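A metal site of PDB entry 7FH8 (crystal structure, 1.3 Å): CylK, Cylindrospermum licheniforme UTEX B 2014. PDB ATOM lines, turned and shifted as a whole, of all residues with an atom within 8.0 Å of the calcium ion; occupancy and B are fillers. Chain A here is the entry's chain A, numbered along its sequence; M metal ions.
OG of Ser 313 is in hydrogen-bond range of N of Gly 315. The backbone carbonyl oxygen (O) of Thr 280 is in hydrogen-bond range of the backbone NH (N) of Asp 293, 2.9 Å away. The side-chain hydroxyl of Thr 335 lies within hydrogen-bond range of the side-chain carboxylate of Glu 317, 2.9 Å away. The side-chain amide nitrogen (NE2) of Gln 310 lies within hydrogen-bond range of the side-chain carboxylate (OD2) of Asp 293, at 2.9 Å. N of Arg 292 is in hydrogen-bond range of OG of Ser 94 (3.0 Å). NH1 of Arg 292 is in hydrogen-bond range of OG of Ser 318 (2.9 Å). N of Gly 290 lies within hydrogen-bond range of OD1 of Asn 288 (2.9 Å). The side-chain carboxylate (OD2) of Asp 293 lies within hydrogen-bond range of the backbone NH (N) of Ile 289, at 2.7 Å.
The calcium ion is bound by the side-chain carboxylate (OD1) of Asp 293 (2.3 Å), the backbone carbonyl oxygen (O) of Gly 315 (2.3 Å), the backbone carbonyl oxygen (O) of Gly 290 (2.3 Å), the side-chain carboxylate (OE2) of Glu 317 (2.3 Å), the backbone carbonyl oxygen (O) of Ser 313 (2.4 Å) and the backbone carbonyl oxygen (O) of Arg 292 (2.4 Å).
Of the 24 residues printed, 6 come within 4 Å of the calcium ion. Along chain A the residues within 4 Å of the calcium ion span positions 290 to 317. The nearest printed residue that does not touch the calcium ion is Thr 314 (4.2 Å).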
ATOM      1  N   SER A  94     -20.106  22.432 -10.907  1.00  0.00           N
ATOM      2  CA  SER A  94     -21.006  22.330 -12.054  1.00  0.00           C
ATOM      3  C   SER A  94     -20.583  23.385 -13.068  1.00  0.00           C
ATOM      4  O   SER A  94     -20.262  24.505 -12.696  1.00  0.00           O
ATOM      5  CB  SER A  94     -22.448  22.593 -11.622  1.00  0.00           C
ATOM      6  OG  SER A  94     -23.356  22.536 -12.714  1.00  0.00           O
ATOM      7  N   ASP A  96     -21.618  25.761 -14.970  1.00  0.00           N
ATOM      8  CA  ASP A  96     -22.711  26.689 -15.208  1.00  0.00           C
ATOM      9  C   ASP A  96     -22.291  28.153 -15.287  1.00  0.00           C
ATOM     10  O   ASP A  96     -23.151  29.017 -15.505  1.00  0.00           O
ATOM     11  CB  ASP A  96     -23.858  26.499 -14.194  1.00  0.00           C
ATOM     12  CG  ASP A  96     -23.433  26.779 -12.750  1.00  0.00           C
ATOM     13  OD1 ASP A  96     -22.303  27.243 -12.513  1.00  0.00           O
ATOM     14  OD2 ASP A  96     -24.257  26.568 -11.845  1.00  0.00           O
ATOM     15  N   THR A 280     -24.831  14.720 -12.151  1.00  0.00           N
ATOM     16  CA  THR A 280     -23.889  14.386 -13.207  1.00  0.00           C
ATOM     17  C   THR A 280     -23.676  15.565 -14.149  1.00  0.00           C
ATOM     18  O   THR A 280     -24.629  16.258 -14.520  1.00  0.00           O
ATOM     19  CB  THR A 280     -24.317  13.152 -14.009  1.00  0.00           C
ATOM     20  OG1 THR A 280     -23.353  12.891 -15.043  1.00  0.00           O
ATOM     21  CG2 THR A 280     -25.697  13.362 -14.657  1.00  0.00           C
ATOM     22  N   GLY A 281     -22.419  15.783 -14.538  1.00  0.00           N
ATOM     23  CA  GLY A 281     -22.097  16.700 -15.611  1.00  0.00           C
ATOM     24  C   GLY A 281     -22.184  16.102 -16.993  1.00  0.00           C
ATOM     25  O   GLY A 281     -21.894  16.793 -17.978  1.00  0.00           O
ATOM     26  N   ASN A 288     -27.648  15.017 -21.416  1.00  0.00           N
ATOM     27  CA  ASN A 288     -27.439  16.143 -20.516  1.00  0.00           C
ATOM     28  C   ASN A 288     -28.231  17.366 -20.979  1.00  0.00           C
ATOM     29  O   ASN A 288     -28.251  17.712 -22.174  1.00  0.00           O
ATOM     30  CB  ASN A 288     -25.945  16.453 -20.431  1.00  0.00           C
ATOM     31  CG  ASN A 288     -25.633  17.565 -19.452  1.00  0.00           C
ATOM     32  OD1 ASN A 288     -25.667  18.741 -19.802  1.00  0.00           O
ATOM     33  ND2 ASN A 288     -25.338  17.186 -18.210  1.00  0.00           N
ATOM     34  N   ILE A 289     -28.898  18.016 -20.033  1.00  0.00           N
ATOM     35  CA  ILE A 289     -29.735  19.176 -20.325  1.00  0.00           C
ATOM     36  C   ILE A 289     -28.927  20.473 -20.277  1.00  0.00           C
ATOM     37  O   ILE A 289     -29.227  21.430 -20.995  1.00  0.00           O
ATOM     38  CB  ILE A 289     -30.905  19.205 -19.314  1.00  0.00           C
ATOM     39  CG1 ILE A 289     -31.692  17.881 -19.336  1.00  0.00           C
ATOM     40  CG2 ILE A 289     -31.835  20.386 -19.573  1.00  0.00           C
ATOM     41  CD1 ILE A 289     -32.528  17.646 -18.078  1.00  0.00           C
ATOM     42  N   GLY A 290     -27.914  20.520 -19.429  1.00  0.00           N
ATOM     43  CA  GLY A 290     -27.018  21.651 -19.312  1.00  0.00           C
ATOM     44  C   GLY A 290     -26.356  21.610 -17.947  1.00  0.00           C
ATOM     45  O   GLY A 290     -27.023  21.319 -16.944  1.00  0.00           O
ATOM     46  N   ALA A 291     -25.048  21.835 -17.907  1.00  0.00           N
ATOM     47  CA  ALA A 291     -24.293  21.823 -16.651  1.00  0.00           C
ATOM     48  C   ALA A 291     -24.571  20.515 -15.892  1.00  0.00           C
ATOM     49  O   ALA A 291     -24.705  19.462 -16.523  1.00  0.00           O
ATOM     50  CB  ALA A 291     -24.644  23.060 -15.812  1.00  0.00           C
ATOM     51  N   ARG A 292     -24.702  20.575 -14.572  1.00  0.00           N
ATOM     52  CA  ARG A 292     -25.047  19.380 -13.817  1.00  0.00           C
ATOM     53  C   ARG A 292     -26.550  19.153 -13.876  1.00  0.00           C
ATOM     54  O   ARG A 292     -27.334  20.103 -13.794  1.00  0.00           O
ATOM     55  CB  ARG A 292     -24.633  19.543 -12.360  1.00  0.00           C
ATOM     56  CG  ARG A 292     -24.964  18.327 -11.498  1.00  0.00           C
ATOM     57  CD  ARG A 292     -24.688  18.570 -10.020  1.00  0.00           C
ATOM     58  NE  ARG A 292     -23.263  18.559  -9.716  1.00  0.00           N
ATOM     59  CZ  ARG A 292     -22.774  18.485  -8.475  1.00  0.00           C
ATOM     60  NH1 ARG A 292     -23.563  18.375  -7.436  1.00  0.00           N
ATOM     61  NH2 ARG A 292     -21.458  18.492  -8.300  1.00  0.00           N
ATOM     62  N   ASP A 293     -26.948  17.882 -14.018  1.00  0.00           N
ATOM     63  CA  ASP A 293     -28.341  17.448 -13.912  1.00  0.00           C
ATOM     64  C   ASP A 293     -28.480  16.469 -12.752  1.00  0.00           C
ATOM     65  O   ASP A 293     -27.510  15.864 -12.297  1.00  0.00           O
ATOM     66  CB  ASP A 293     -28.795  16.691 -15.163  1.00  0.00           C
ATOM     67  CG  ASP A 293     -28.829  17.550 -16.432  1.00  0.00           C
ATOM     68  OD1 ASP A 293     -28.906  18.791 -16.339  1.00  0.00           O
ATOM     69  OD2 ASP A 293     -28.814  16.940 -17.524  1.00  0.00           O
ATOM     70  N   ALA A 294     -29.725  16.292 -12.322  1.00  0.00           N
ATOM     71  CA  ALA A 294     -30.047  15.261 -11.337  1.00  0.00           C
ATOM     72  C   ALA A 294     -30.273  13.937 -12.047  1.00  0.00           C
ATOM     73  O   ALA A 294     -30.730  13.900 -13.188  1.00  0.00           O
ATOM     74  CB  ALA A 294     -31.314  15.648 -10.574  1.00  0.00           C
ATOM     75  N   GLN A 310     -32.817  10.943 -15.848  1.00  0.00           N
ATOM     76  CA  GLN A 310     -32.048  12.158 -15.660  1.00  0.00           C
ATOM     77  C   GLN A 310     -33.002  13.319 -15.898  1.00  0.00           C
ATOM     78  O   GLN A 310     -33.822  13.274 -16.817  1.00  0.00           O
ATOM     79  CB  GLN A 310     -30.853  12.186 -16.629  1.00  0.00           C
ATOM     80  CG  GLN A 310     -29.947  13.410 -16.497  1.00  0.00           C
ATOM     81  CD  GLN A 310     -28.533  13.142 -16.996  1.00  0.00           C
ATOM     82  OE1 GLN A 310     -28.019  12.022 -16.928  1.00  0.00           O
ATOM     83  NE2 GLN A 310     -27.891  14.190 -17.501  1.00  0.00           N
ATOM     84  N   PHE A 311     -32.902  14.352 -15.072  1.00  0.00           N
ATOM     85  CA  PHE A 311     -33.858  15.442 -15.143  1.00  0.00           C
ATOM     86  C   PHE A 311     -33.234  16.724 -14.602  1.00  0.00           C
ATOM     87  O   PHE A 311     -32.217  16.691 -13.901  1.00  0.00           O
ATOM     88  CB  PHE A 311     -35.163  15.117 -14.394  1.00  0.00           C
ATOM     89  CG  PHE A 311     -35.018  15.083 -12.889  1.00  0.00           C
ATOM     90  CD1 PHE A 311     -34.632  13.921 -12.235  1.00  0.00           C
ATOM     91  CD2 PHE A 311     -35.279  16.225 -12.137  1.00  0.00           C
ATOM     92  CE1 PHE A 311     -34.494  13.903 -10.850  1.00  0.00           C
ATOM     93  CE2 PHE A 311     -35.155  16.206 -10.750  1.00  0.00           C
ATOM     94  CZ  PHE A 311     -34.762  15.038 -10.107  1.00  0.00           C
ATOM     95  N   GLY A 312     -33.873  17.846 -14.908  1.00  0.00           N
ATOM     96  CA  GLY A 312     -33.398  19.127 -14.420  1.00  0.00           C
ATOM     97  C   GLY A 312     -33.695  20.254 -15.370  1.00  0.00           C
ATOM     98  O   GLY A 312     -34.814  20.367 -15.902  1.00  0.00           O
ATOM     99  N   SER A 313     -32.687  21.092 -15.597  1.00  0.00           N
ATOM    100  CA  SER A 313     -32.828  22.330 -16.345  1.00  0.00           C
ATOM    101  C   SER A 313     -31.493  22.609 -17.010  1.00  0.00           C
ATOM    102  O   SER A 313     -30.511  21.890 -16.806  1.00  0.00           O
ATOM    103  CB  SER A 313     -33.195  23.492 -15.408  1.00  0.00           C
ATOM    104  OG  SER A 313     -32.058  23.885 -14.641  1.00  0.00           O
ATOM    105  N   THR A 314     -31.450  23.694 -17.779  1.00  0.00           N
ATOM    106  CA  THR A 314     -30.176  24.135 -18.335  1.00  0.00           C
ATOM    107  C   THR A 314     -29.238  24.684 -17.264  1.00  0.00           C
ATOM    108  O   THR A 314     -28.049  24.892 -17.555  1.00  0.00           O
ATOM    109  CB  THR A 314     -30.391  25.184 -19.420  1.00  0.00           C
ATOM    110  OG1 THR A 314     -31.132  26.273 -18.880  1.00  0.00           O
ATOM    111  CG2 THR A 314     -31.151  24.573 -20.597  1.00  0.00           C
ATOM    112  N   GLY A 315     -29.757  24.961 -16.067  1.00  0.00           N
ATOM    113  CA  GLY A 315     -28.950  25.323 -14.923  1.00  0.00           C
ATOM    114  C   GLY A 315     -28.446  24.097 -14.185  1.00  0.00           C
ATOM    115  O   GLY A 315     -28.358  23.002 -14.743  1.00  0.00           O
ATOM    116  N   THR A 316     -28.124  24.277 -12.908  1.00  0.00           N
ATOM    117  CA  THR A 316     -27.516  23.238 -12.099  1.00  0.00           C
ATOM    118  C   THR A 316     -28.520  22.674 -11.106  1.00  0.00           C
ATOM    119  O   THR A 316     -29.209  23.437 -10.423  1.00  0.00           O
ATOM    120  CB  THR A 316     -26.344  23.842 -11.322  1.00  0.00           C
ATOM    121  OG1 THR A 316     -25.334  24.187 -12.269  1.00  0.00           O
ATOM    122  CG2 THR A 316     -25.791  22.874 -10.259  1.00  0.00           C
ATOM    123  N   GLU A 317     -28.584  21.355 -10.997  1.00  0.00           N
ATOM    124  CA  GLU A 317     -29.350  20.724  -9.945  1.00  0.00           C
ATOM    125  C   GLU A 317     -28.742  19.362  -9.642  1.00  0.00           C
ATOM    126  O   GLU A 317     -28.020  18.786 -10.448  1.00  0.00           O
ATOM    127  CB  GLU A 317     -30.825  20.571 -10.335  1.00  0.00           C
ATOM    128  CG  GLU A 317     -31.034  19.951 -11.735  1.00  0.00           C
ATOM    129  CD  GLU A 317     -30.968  20.975 -12.853  1.00  0.00           C
ATOM    130  OE1 GLU A 317     -31.455  22.103 -12.641  1.00  0.00           O
ATOM    131  OE2 GLU A 317     -30.454  20.652 -13.941  1.00  0.00           O
ATOM    132  N   SER A 318     -29.086  18.840  -8.459  1.00  0.00           N
ATOM    133  CA  SER A 318     -28.671  17.527  -8.010  1.00  0.00           C
ATOM    134  C   SER A 318     -29.827  16.886  -7.278  1.00  0.00           C
ATOM    135  O   SER A 318     -30.698  17.572  -6.730  1.00  0.00           O
ATOM    136  CB  SER A 318     -27.524  17.627  -6.982  1.00  0.00           C
ATOM    137  OG  SER A 318     -26.446  18.394  -7.464  1.00  0.00           O
ATOM    138  N   THR A 335     -31.885  23.583  -7.147  1.00  0.00           N
ATOM    139  CA  THR A 335     -31.675  23.940  -8.539  1.00  0.00           C
ATOM    140  C   THR A 335     -31.307  25.418  -8.611  1.00  0.00           C
ATOM    141  O   THR A 335     -31.727  26.217  -7.773  1.00  0.00           O
ATOM    142  CB  THR A 335     -32.909  23.644  -9.419  1.00  0.00           C
ATOM    143  OG1 THR A 335     -32.614  23.974 -10.781  1.00  0.00           O
ATOM    144  CG2 THR A 335     -34.130  24.443  -8.975  1.00  0.00           C
ATOM    145  N   THR A 336     -30.527  25.761  -9.633  1.00  0.00           N
ATOM    146  CA  THR A 336     -30.290  27.158  -9.978  1.00  0.00           C
ATOM    147  C   THR A 336     -31.174  27.623 -11.108  1.00  0.00           C
ATOM    148  O   THR A 336     -31.139  28.809 -11.466  1.00  0.00           O
ATOM    149  CB  THR A 336     -28.830  27.384 -10.409  1.00  0.00           C
ATOM    150  OG1 THR A 336     -28.622  26.788 -11.704  1.00  0.00           O
ATOM    151  CG2 THR A 336     -27.851  26.770  -9.391  1.00  0.00           C
ATOM    152  N   GLY A 337     -31.963  26.717 -11.697  1.00  0.00           N
ATOM    153  CA  GLY A 337     -32.757  27.025 -12.867  1.00  0.00           C
ATOM    154  C   GLY A 337     -34.245  26.917 -12.617  1.00  0.00           C
ATOM    155  O   GLY A 337     -34.709  27.027 -11.468  1.00  0.00           O
ATOM    156  N   LEU A 339     -37.300  24.320 -13.106  1.00  0.00           N
ATOM    157  CA  LEU A 339     -37.615  22.945 -13.426  1.00  0.00           C
ATOM    158  C   LEU A 339     -38.915  22.877 -14.223  1.00  0.00           C
ATOM    159  O   LEU A 339     -39.687  23.841 -14.293  1.00  0.00           O
ATOM    160  CB  LEU A 339     -37.720  22.117 -12.139  1.00  0.00           C
ATOM    161  CG  LEU A 339     -36.393  22.090 -11.352  1.00  0.00           C
ATOM    162  CD1 LEU A 339     -36.629  21.577  -9.938  1.00  0.00           C
ATOM    163  CD2 LEU A 339     -35.312  21.303 -12.081  1.00  0.00           C
HETATM  164 CA    CA M   1     -28.784  20.900 -15.514  1.00  0.00          CA
